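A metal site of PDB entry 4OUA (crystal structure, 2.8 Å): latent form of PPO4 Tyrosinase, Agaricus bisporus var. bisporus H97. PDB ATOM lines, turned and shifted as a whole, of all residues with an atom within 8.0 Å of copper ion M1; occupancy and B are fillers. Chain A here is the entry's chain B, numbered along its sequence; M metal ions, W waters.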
ATOM      1  N   ILE A  55      20.989  -6.863 -15.729  1.00  0.00           N
ATOM      2  CA  ILE A  55      20.266  -7.946 -15.054  1.00  0.00           C
ATOM      3  C   ILE A  55      18.770  -7.883 -15.339  1.00  0.00           C
ATOM      4  O   ILE A  55      18.133  -8.913 -15.565  1.00  0.00           O
ATOM      5  CB  ILE A  55      20.494  -7.897 -13.536  1.00  0.00           C
ATOM      6  CG1 ILE A  55      21.955  -8.176 -13.206  1.00  0.00           C
ATOM      7  CG2 ILE A  55      19.577  -8.897 -12.833  1.00  0.00           C
ATOM      8  CD1 ILE A  55      22.276  -8.140 -11.726  1.00  0.00           C
ATOM      9  N   HIS A  56      18.218  -6.671 -15.314  1.00  0.00           N
ATOM     10  CA  HIS A  56      16.783  -6.467 -15.497  1.00  0.00           C
ATOM     11  C   HIS A  56      16.281  -7.089 -16.795  1.00  0.00           C
ATOM     12  O   HIS A  56      15.569  -8.091 -16.787  1.00  0.00           O
ATOM     13  CB  HIS A  56      16.455  -4.976 -15.470  1.00  0.00           C
ATOM     14  CG  HIS A  56      15.017  -4.680 -15.183  1.00  0.00           C
ATOM     15  ND1 HIS A  56      14.144  -4.214 -16.151  1.00  0.00           N
ATOM     16  CD2 HIS A  56      14.287  -4.783 -14.046  1.00  0.00           C
ATOM     17  CE1 HIS A  56      12.951  -4.034 -15.624  1.00  0.00           C
ATOM     18  NE2 HIS A  56      13.012  -4.376 -14.341  1.00  0.00           N
ATOM     19  N   GLY A  57      16.659  -6.487 -17.918  1.00  0.00           N
ATOM     20  CA  GLY A  57      16.268  -6.988 -19.224  1.00  0.00           C
ATOM     21  C   GLY A  57      17.471  -7.465 -20.018  1.00  0.00           C
ATOM     22  O   GLY A  57      18.072  -8.491 -19.691  1.00  0.00           O
ATOM     23  N   TYR A  78      16.078 -11.081 -16.102  1.00  0.00           N
ATOM     24  CA  TYR A  78      15.956 -11.680 -14.768  1.00  0.00           C
ATOM     25  C   TYR A  78      14.735 -11.158 -14.026  1.00  0.00           C
ATOM     26  O   TYR A  78      14.158 -11.870 -13.201  1.00  0.00           O
ATOM     27  CB  TYR A  78      17.197 -11.395 -13.928  1.00  0.00           C
ATOM     28  CG  TYR A  78      18.319 -12.402 -14.053  1.00  0.00           C
ATOM     29  CD1 TYR A  78      18.206 -13.664 -13.479  1.00  0.00           C
ATOM     30  CD2 TYR A  78      19.500 -12.084 -14.706  1.00  0.00           C
ATOM     31  CE1 TYR A  78      19.233 -14.586 -13.586  1.00  0.00           C
ATOM     32  CE2 TYR A  78      20.530 -12.992 -14.813  1.00  0.00           C
ATOM     33  CZ  TYR A  78      20.392 -14.242 -14.255  1.00  0.00           C
ATOM     34  OH  TYR A  78      21.418 -15.149 -14.349  1.00  0.00           O
ATOM     35  N   CYS A  79      14.345  -9.914 -14.312  1.00  0.00           N
ATOM     36  CA  CYS A  79      13.285  -9.258 -13.559  1.00  0.00           C
ATOM     37  C   CYS A  79      11.963 -10.000 -13.677  1.00  0.00           C
ATOM     38  O   CYS A  79      11.640 -10.538 -14.739  1.00  0.00           O
ATOM     39  CB  CYS A  79      13.126  -7.800 -14.011  1.00  0.00           C
ATOM     40  SG  CYS A  79      12.338  -7.591 -15.620  1.00  0.00           S
ATOM     41  N   THR A  80      11.208 -10.026 -12.582  1.00  0.00           N
ATOM     42  CA  THR A  80       9.934 -10.716 -12.544  1.00  0.00           C
ATOM     43  C   THR A  80       8.778  -9.728 -12.567  1.00  0.00           C
ATOM     44  O   THR A  80       8.591  -8.958 -11.636  1.00  0.00           O
ATOM     45  CB  THR A  80       9.809 -11.598 -11.283  1.00  0.00           C
ATOM     46  OG1 THR A  80       9.778 -10.768 -10.122  1.00  0.00           O
ATOM     47  CG2 THR A  80      10.993 -12.554 -11.188  1.00  0.00           C
ATOM     48  N   HIS A  81       8.010  -9.755 -13.649  1.00  0.00           N
ATOM     49  CA  HIS A  81       6.887  -8.842 -13.796  1.00  0.00           C
ATOM     50  C   HIS A  81       5.580  -9.597 -14.049  1.00  0.00           C
ATOM     51  O   HIS A  81       5.585 -10.674 -14.643  1.00  0.00           O
ATOM     52  CB  HIS A  81       7.168  -7.845 -14.934  1.00  0.00           C
ATOM     53  CG  HIS A  81       8.513  -7.195 -14.847  1.00  0.00           C
ATOM     54  ND1 HIS A  81       9.642  -7.731 -15.429  1.00  0.00           N
ATOM     55  CD2 HIS A  81       8.908  -6.055 -14.233  1.00  0.00           C
ATOM     56  CE1 HIS A  81      10.678  -6.942 -15.174  1.00  0.00           C
ATOM     57  NE2 HIS A  81      10.254  -5.919 -14.456  1.00  0.00           N
ATOM     58  N   PHE A  86       7.222 -10.136  -7.922  1.00  0.00           N
ATOM     59  CA  PHE A  86       7.577  -8.783  -8.355  1.00  0.00           C
ATOM     60  C   PHE A  86       8.135  -7.917  -7.224  1.00  0.00           C
ATOM     61  O   PHE A  86       9.237  -7.381  -7.357  1.00  0.00           O
ATOM     62  CB  PHE A  86       6.363  -8.079  -8.982  1.00  0.00           C
ATOM     63  CG  PHE A  86       6.598  -6.625  -9.265  1.00  0.00           C
ATOM     64  CD1 PHE A  86       7.264  -6.228 -10.422  1.00  0.00           C
ATOM     65  CD2 PHE A  86       6.139  -5.650  -8.391  1.00  0.00           C
ATOM     66  CE1 PHE A  86       7.482  -4.886 -10.686  1.00  0.00           C
ATOM     67  CE2 PHE A  86       6.357  -4.307  -8.655  1.00  0.00           C
ATOM     68  CZ  PHE A  86       7.027  -3.932  -9.802  1.00  0.00           C
ATOM     69  N   TRP A  89      11.540  -9.660  -5.550  1.00  0.00           N
ATOM     70  CA  TRP A  89      12.679  -9.773  -6.459  1.00  0.00           C
ATOM     71  C   TRP A  89      13.361  -8.423  -6.637  1.00  0.00           C
ATOM     72  O   TRP A  89      14.591  -8.337  -6.646  1.00  0.00           O
ATOM     73  CB  TRP A  89      12.241 -10.323  -7.818  1.00  0.00           C
ATOM     74  CG  TRP A  89      13.398 -10.491  -8.754  1.00  0.00           C
ATOM     75  CD1 TRP A  89      14.129 -11.629  -8.971  1.00  0.00           C
ATOM     76  CD2 TRP A  89      13.976  -9.482  -9.597  1.00  0.00           C
ATOM     77  NE1 TRP A  89      15.108 -11.391  -9.895  1.00  0.00           N
ATOM     78  CE2 TRP A  89      15.041 -10.080 -10.294  1.00  0.00           C
ATOM     79  CE3 TRP A  89      13.695  -8.137  -9.824  1.00  0.00           C
ATOM     80  CZ2 TRP A  89      15.822  -9.376 -11.202  1.00  0.00           C
ATOM     81  CZ3 TRP A  89      14.476  -7.433 -10.731  1.00  0.00           C
ATOM     82  CH2 TRP A  89      15.528  -8.056 -11.401  1.00  0.00           C
ATOM     83  N   HIS A  90      12.559  -7.373  -6.809  1.00  0.00           N
ATOM     84  CA  HIS A  90      13.102  -6.038  -6.995  1.00  0.00           C
ATOM     85  C   HIS A  90      13.725  -5.492  -5.724  1.00  0.00           C
ATOM     86  O   HIS A  90      14.639  -4.664  -5.779  1.00  0.00           O
ATOM     87  CB  HIS A  90      12.007  -5.089  -7.499  1.00  0.00           C
ATOM     88  CG  HIS A  90      11.618  -5.333  -8.929  1.00  0.00           C
ATOM     89  ND1 HIS A  90      10.796  -6.365  -9.317  1.00  0.00           N
ATOM     90  CD2 HIS A  90      11.939  -4.669 -10.065  1.00  0.00           C
ATOM     91  CE1 HIS A  90      10.629  -6.327 -10.627  1.00  0.00           C
ATOM     92  NE2 HIS A  90      11.313  -5.303 -11.101  1.00  0.00           N
ATOM     93  N   TYR A  93      17.035  -6.656  -5.635  1.00  0.00           N
ATOM     94  CA  TYR A  93      17.651  -6.068  -6.815  1.00  0.00           C
ATOM     95  C   TYR A  93      18.217  -4.676  -6.536  1.00  0.00           C
ATOM     96  O   TYR A  93      19.254  -4.303  -7.064  1.00  0.00           O
ATOM     97  CB  TYR A  93      16.650  -5.985  -7.965  1.00  0.00           C
ATOM     98  CG  TYR A  93      17.239  -5.510  -9.275  1.00  0.00           C
ATOM     99  CD1 TYR A  93      18.519  -5.885  -9.651  1.00  0.00           C
ATOM    100  CD2 TYR A  93      16.509  -4.702 -10.136  1.00  0.00           C
ATOM    101  CE1 TYR A  93      19.067  -5.457 -10.852  1.00  0.00           C
ATOM    102  CE2 TYR A  93      17.047  -4.273 -11.340  1.00  0.00           C
ATOM    103  CZ  TYR A  93      18.329  -4.654 -11.693  1.00  0.00           C
ATOM    104  OH  TYR A  93      18.863  -4.223 -12.882  1.00  0.00           O
ATOM    105  N   GLU A 247       2.613  -2.822  -8.715  1.00  0.00           N
ATOM    106  CA  GLU A 247       3.218  -2.828 -10.040  1.00  0.00           C
ATOM    107  C   GLU A 247       2.524  -1.835 -10.973  1.00  0.00           C
ATOM    108  O   GLU A 247       3.173  -1.187 -11.795  1.00  0.00           O
ATOM    109  CB  GLU A 247       3.180  -4.229 -10.635  1.00  0.00           C
ATOM    110  CG  GLU A 247       4.051  -4.418 -11.871  1.00  0.00           C
ATOM    111  CD  GLU A 247       3.992  -5.842 -12.410  1.00  0.00           C
ATOM    112  OE1 GLU A 247       2.999  -6.533 -12.138  1.00  0.00           O
ATOM    113  OE2 GLU A 247       4.945  -6.250 -13.104  1.00  0.00           O
ATOM    114  N   HIS A 250       3.558   1.444 -10.224  1.00  0.00           N
ATOM    115  CA  HIS A 250       4.970   1.376 -10.589  1.00  0.00           C
ATOM    116  C   HIS A 250       5.186   1.626 -12.081  1.00  0.00           C
ATOM    117  O   HIS A 250       6.128   2.310 -12.471  1.00  0.00           O
ATOM    118  CB  HIS A 250       5.526   0.007 -10.195  1.00  0.00           C
ATOM    119  CG  HIS A 250       6.704  -0.422 -11.015  1.00  0.00           C
ATOM    120  ND1 HIS A 250       6.586  -1.227 -12.123  1.00  0.00           N
ATOM    121  CD2 HIS A 250       8.031  -0.165 -10.878  1.00  0.00           C
ATOM    122  CE1 HIS A 250       7.780  -1.443 -12.640  1.00  0.00           C
ATOM    123  NE2 HIS A 250       8.672  -0.814 -11.897  1.00  0.00           N
ATOM    124  N   ASP A 251       4.303   1.072 -12.910  1.00  0.00           N
ATOM    125  CA  ASP A 251       4.438   1.196 -14.355  1.00  0.00           C
ATOM    126  C   ASP A 251       4.226   2.629 -14.828  1.00  0.00           C
ATOM    127  O   ASP A 251       4.781   3.053 -15.842  1.00  0.00           O
ATOM    128  CB  ASP A 251       3.457   0.268 -15.069  1.00  0.00           C
ATOM    129  CG  ASP A 251       3.656  -1.186 -14.709  1.00  0.00           C
ATOM    130  OD1 ASP A 251       2.677  -1.954 -14.788  1.00  0.00           O
ATOM    131  OD2 ASP A 251       4.785  -1.568 -14.332  1.00  0.00           O
ATOM    132  N   HIS A 254       7.361   4.596 -15.165  1.00  0.00           N
ATOM    133  CA  HIS A 254       8.145   4.153 -16.316  1.00  0.00           C
ATOM    134  C   HIS A 254       7.647   4.802 -17.599  1.00  0.00           C
ATOM    135  O   HIS A 254       8.434   5.167 -18.470  1.00  0.00           O
ATOM    136  CB  HIS A 254       8.096   2.637 -16.447  1.00  0.00           C
ATOM    137  CG  HIS A 254       8.971   1.924 -15.472  1.00  0.00           C
ATOM    138  ND1 HIS A 254      10.323   1.756 -15.669  1.00  0.00           N
ATOM    139  CD2 HIS A 254       8.691   1.318 -14.293  1.00  0.00           C
ATOM    140  CE1 HIS A 254      10.844   1.090 -14.650  1.00  0.00           C
ATOM    141  NE2 HIS A 254       9.868   0.813 -13.803  1.00  0.00           N
ATOM    142  N   ALA A 269      11.053  -2.428 -20.783  1.00  0.00           N
ATOM    143  CA  ALA A 269      11.562  -3.272 -19.701  1.00  0.00           C
ATOM    144  C   ALA A 269      12.941  -3.859 -19.981  1.00  0.00           C
ATOM    145  O   ALA A 269      13.647  -4.278 -19.063  1.00  0.00           O
ATOM    146  CB  ALA A 269      10.581  -4.391 -19.398  1.00  0.00           C
ATOM    147  N   ALA A 272      15.043  -0.243 -19.491  1.00  0.00           N
ATOM    148  CA  ALA A 272      14.647   0.710 -18.451  1.00  0.00           C
ATOM    149  C   ALA A 272      15.670   0.852 -17.329  1.00  0.00           C
ATOM    150  O   ALA A 272      15.817   1.926 -16.750  1.00  0.00           O
ATOM    151  CB  ALA A 272      13.291   0.310 -17.870  1.00  0.00           C
ATOM    152  N   ALA A 273      16.381  -0.233 -17.017  1.00  0.00           N
ATOM    153  CA  ALA A 273      17.312  -0.231 -15.895  1.00  0.00           C
ATOM    154  C   ALA A 273      18.562   0.602 -16.187  1.00  0.00           C
ATOM    155  O   ALA A 273      19.281   0.990 -15.274  1.00  0.00           O
ATOM    156  CB  ALA A 273      17.697  -1.659 -15.536  1.00  0.00           C
ATOM    157  N   PHE A 278      16.172   5.007 -12.772  1.00  0.00           N
ATOM    158  CA  PHE A 278      15.513   3.734 -12.513  1.00  0.00           C
ATOM    159  C   PHE A 278      15.554   3.358 -11.041  1.00  0.00           C
ATOM    160  O   PHE A 278      14.556   2.935 -10.468  1.00  0.00           O
ATOM    161  CB  PHE A 278      16.167   2.646 -13.367  1.00  0.00           C
ATOM    162  CG  PHE A 278      15.573   1.271 -13.184  1.00  0.00           C
ATOM    163  CD1 PHE A 278      16.050   0.425 -12.207  1.00  0.00           C
ATOM    164  CD2 PHE A 278      14.568   0.829 -14.026  1.00  0.00           C
ATOM    165  CE1 PHE A 278      15.519  -0.842 -12.052  1.00  0.00           C
ATOM    166  CE2 PHE A 278      14.027  -0.435 -13.874  1.00  0.00           C
ATOM    167  CZ  PHE A 278      14.512  -1.276 -12.887  1.00  0.00           C
ATOM    168  N   HIS A 282      12.725   2.659  -7.990  1.00  0.00           N
ATOM    169  CA  HIS A 282      12.506   1.392  -7.313  1.00  0.00           C
ATOM    170  C   HIS A 282      12.866   1.449  -5.839  1.00  0.00           C
ATOM    171  O   HIS A 282      12.432   0.612  -5.044  1.00  0.00           O
ATOM    172  CB  HIS A 282      13.286   0.275  -8.004  1.00  0.00           C
ATOM    173  CG  HIS A 282      12.609  -0.251  -9.226  1.00  0.00           C
ATOM    174  ND1 HIS A 282      11.626  -1.217  -9.171  1.00  0.00           N
ATOM    175  CD2 HIS A 282      12.763   0.060 -10.535  1.00  0.00           C
ATOM    176  CE1 HIS A 282      11.207  -1.479 -10.401  1.00  0.00           C
ATOM    177  NE2 HIS A 282      11.882  -0.722 -11.240  1.00  0.00           N
ATOM    178  N   GLU A 308       4.786 -14.158 -18.182  1.00  0.00           N
ATOM    179  CA  GLU A 308       5.500 -13.619 -19.330  1.00  0.00           C
ATOM    180  C   GLU A 308       6.861 -14.280 -19.528  1.00  0.00           C
ATOM    181  O   GLU A 308       7.360 -14.360 -20.655  1.00  0.00           O
ATOM    182  CB  GLU A 308       5.667 -12.105 -19.202  1.00  0.00           C
ATOM    183  CG  GLU A 308       6.590 -11.660 -18.081  1.00  0.00           C
ATOM    184  CD  GLU A 308       6.693 -10.148 -17.986  1.00  0.00           C
ATOM    185  OE1 GLU A 308       5.768  -9.457 -18.487  1.00  0.00           O
ATOM    186  OE2 GLU A 308       7.680  -9.651 -17.404  1.00  0.00           O
ATOM    187  N   PHE A 453       3.844  -0.995 -19.115  1.00  0.00           N
ATOM    188  CA  PHE A 453       5.274  -1.254 -19.097  1.00  0.00           C
ATOM    189  C   PHE A 453       5.553  -2.660 -19.618  1.00  0.00           C
ATOM    190  O   PHE A 453       5.366  -3.643 -18.896  1.00  0.00           O
ATOM    191  CB  PHE A 453       5.833  -1.081 -17.680  1.00  0.00           C
ATOM    192  CG  PHE A 453       7.330  -1.149 -17.616  1.00  0.00           C
ATOM    193  CD1 PHE A 453       8.118  -0.416 -18.494  1.00  0.00           C
ATOM    194  CD2 PHE A 453       7.960  -1.926 -16.646  1.00  0.00           C
ATOM    195  CE1 PHE A 453       9.500  -0.468 -18.427  1.00  0.00           C
ATOM    196  CE2 PHE A 453       9.342  -1.978 -16.578  1.00  0.00           C
ATOM    197  CZ  PHE A 453      10.108  -1.255 -17.462  1.00  0.00           C
HETATM  198 CU    CU M   1      11.600  -5.152 -13.111  1.00  0.00          CU
HETATM  199 CU    CU M   2      10.549  -0.621 -12.690  1.00  0.00          CU
HETATM  200  O   HOH W   1      11.045  -2.894 -12.879  1.00  0.00           O
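Residues that only touch copper ion M1: Cys 79 (3.2 Å).
Four residues have an atom within 4 Å of copper ion M1: His 56, Cys 79, His 81 and His 90.
O of His 56 sits at hydrogen-bond distance from N of Cys 79 (3.3 Å).
O of His 56 sits at hydrogen-bond distance from N of Tyr 78 (3.1 Å).
The backbone carbonyl oxygen of Ala 269 is in hydrogen-bond range of a ring nitrogen (ND1) of His 56 (3.0 Å).
A ring nitrogen (ND1) of His 81 sits close to the side-chain carboxylate of Glu 308 (3.4 Å).
SG of Cys 79 is covalently linked to CE1 of His 81.
A ring nitrogen (ND1) of His 90 lies within hydrogen-bond range of the backbone carbonyl oxygen of Phe 86, 2.7 Å away.
A ring nitrogen (NE2) of His 56 binds copper ion M1 (2.0 Å).
Copper ion M1 is bound by NE2 of His 90, at 2.0 Å.
NE2 of His 81 binds copper ion M1.
Copper ion M1 is bound by water W1 (2.3 Å).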
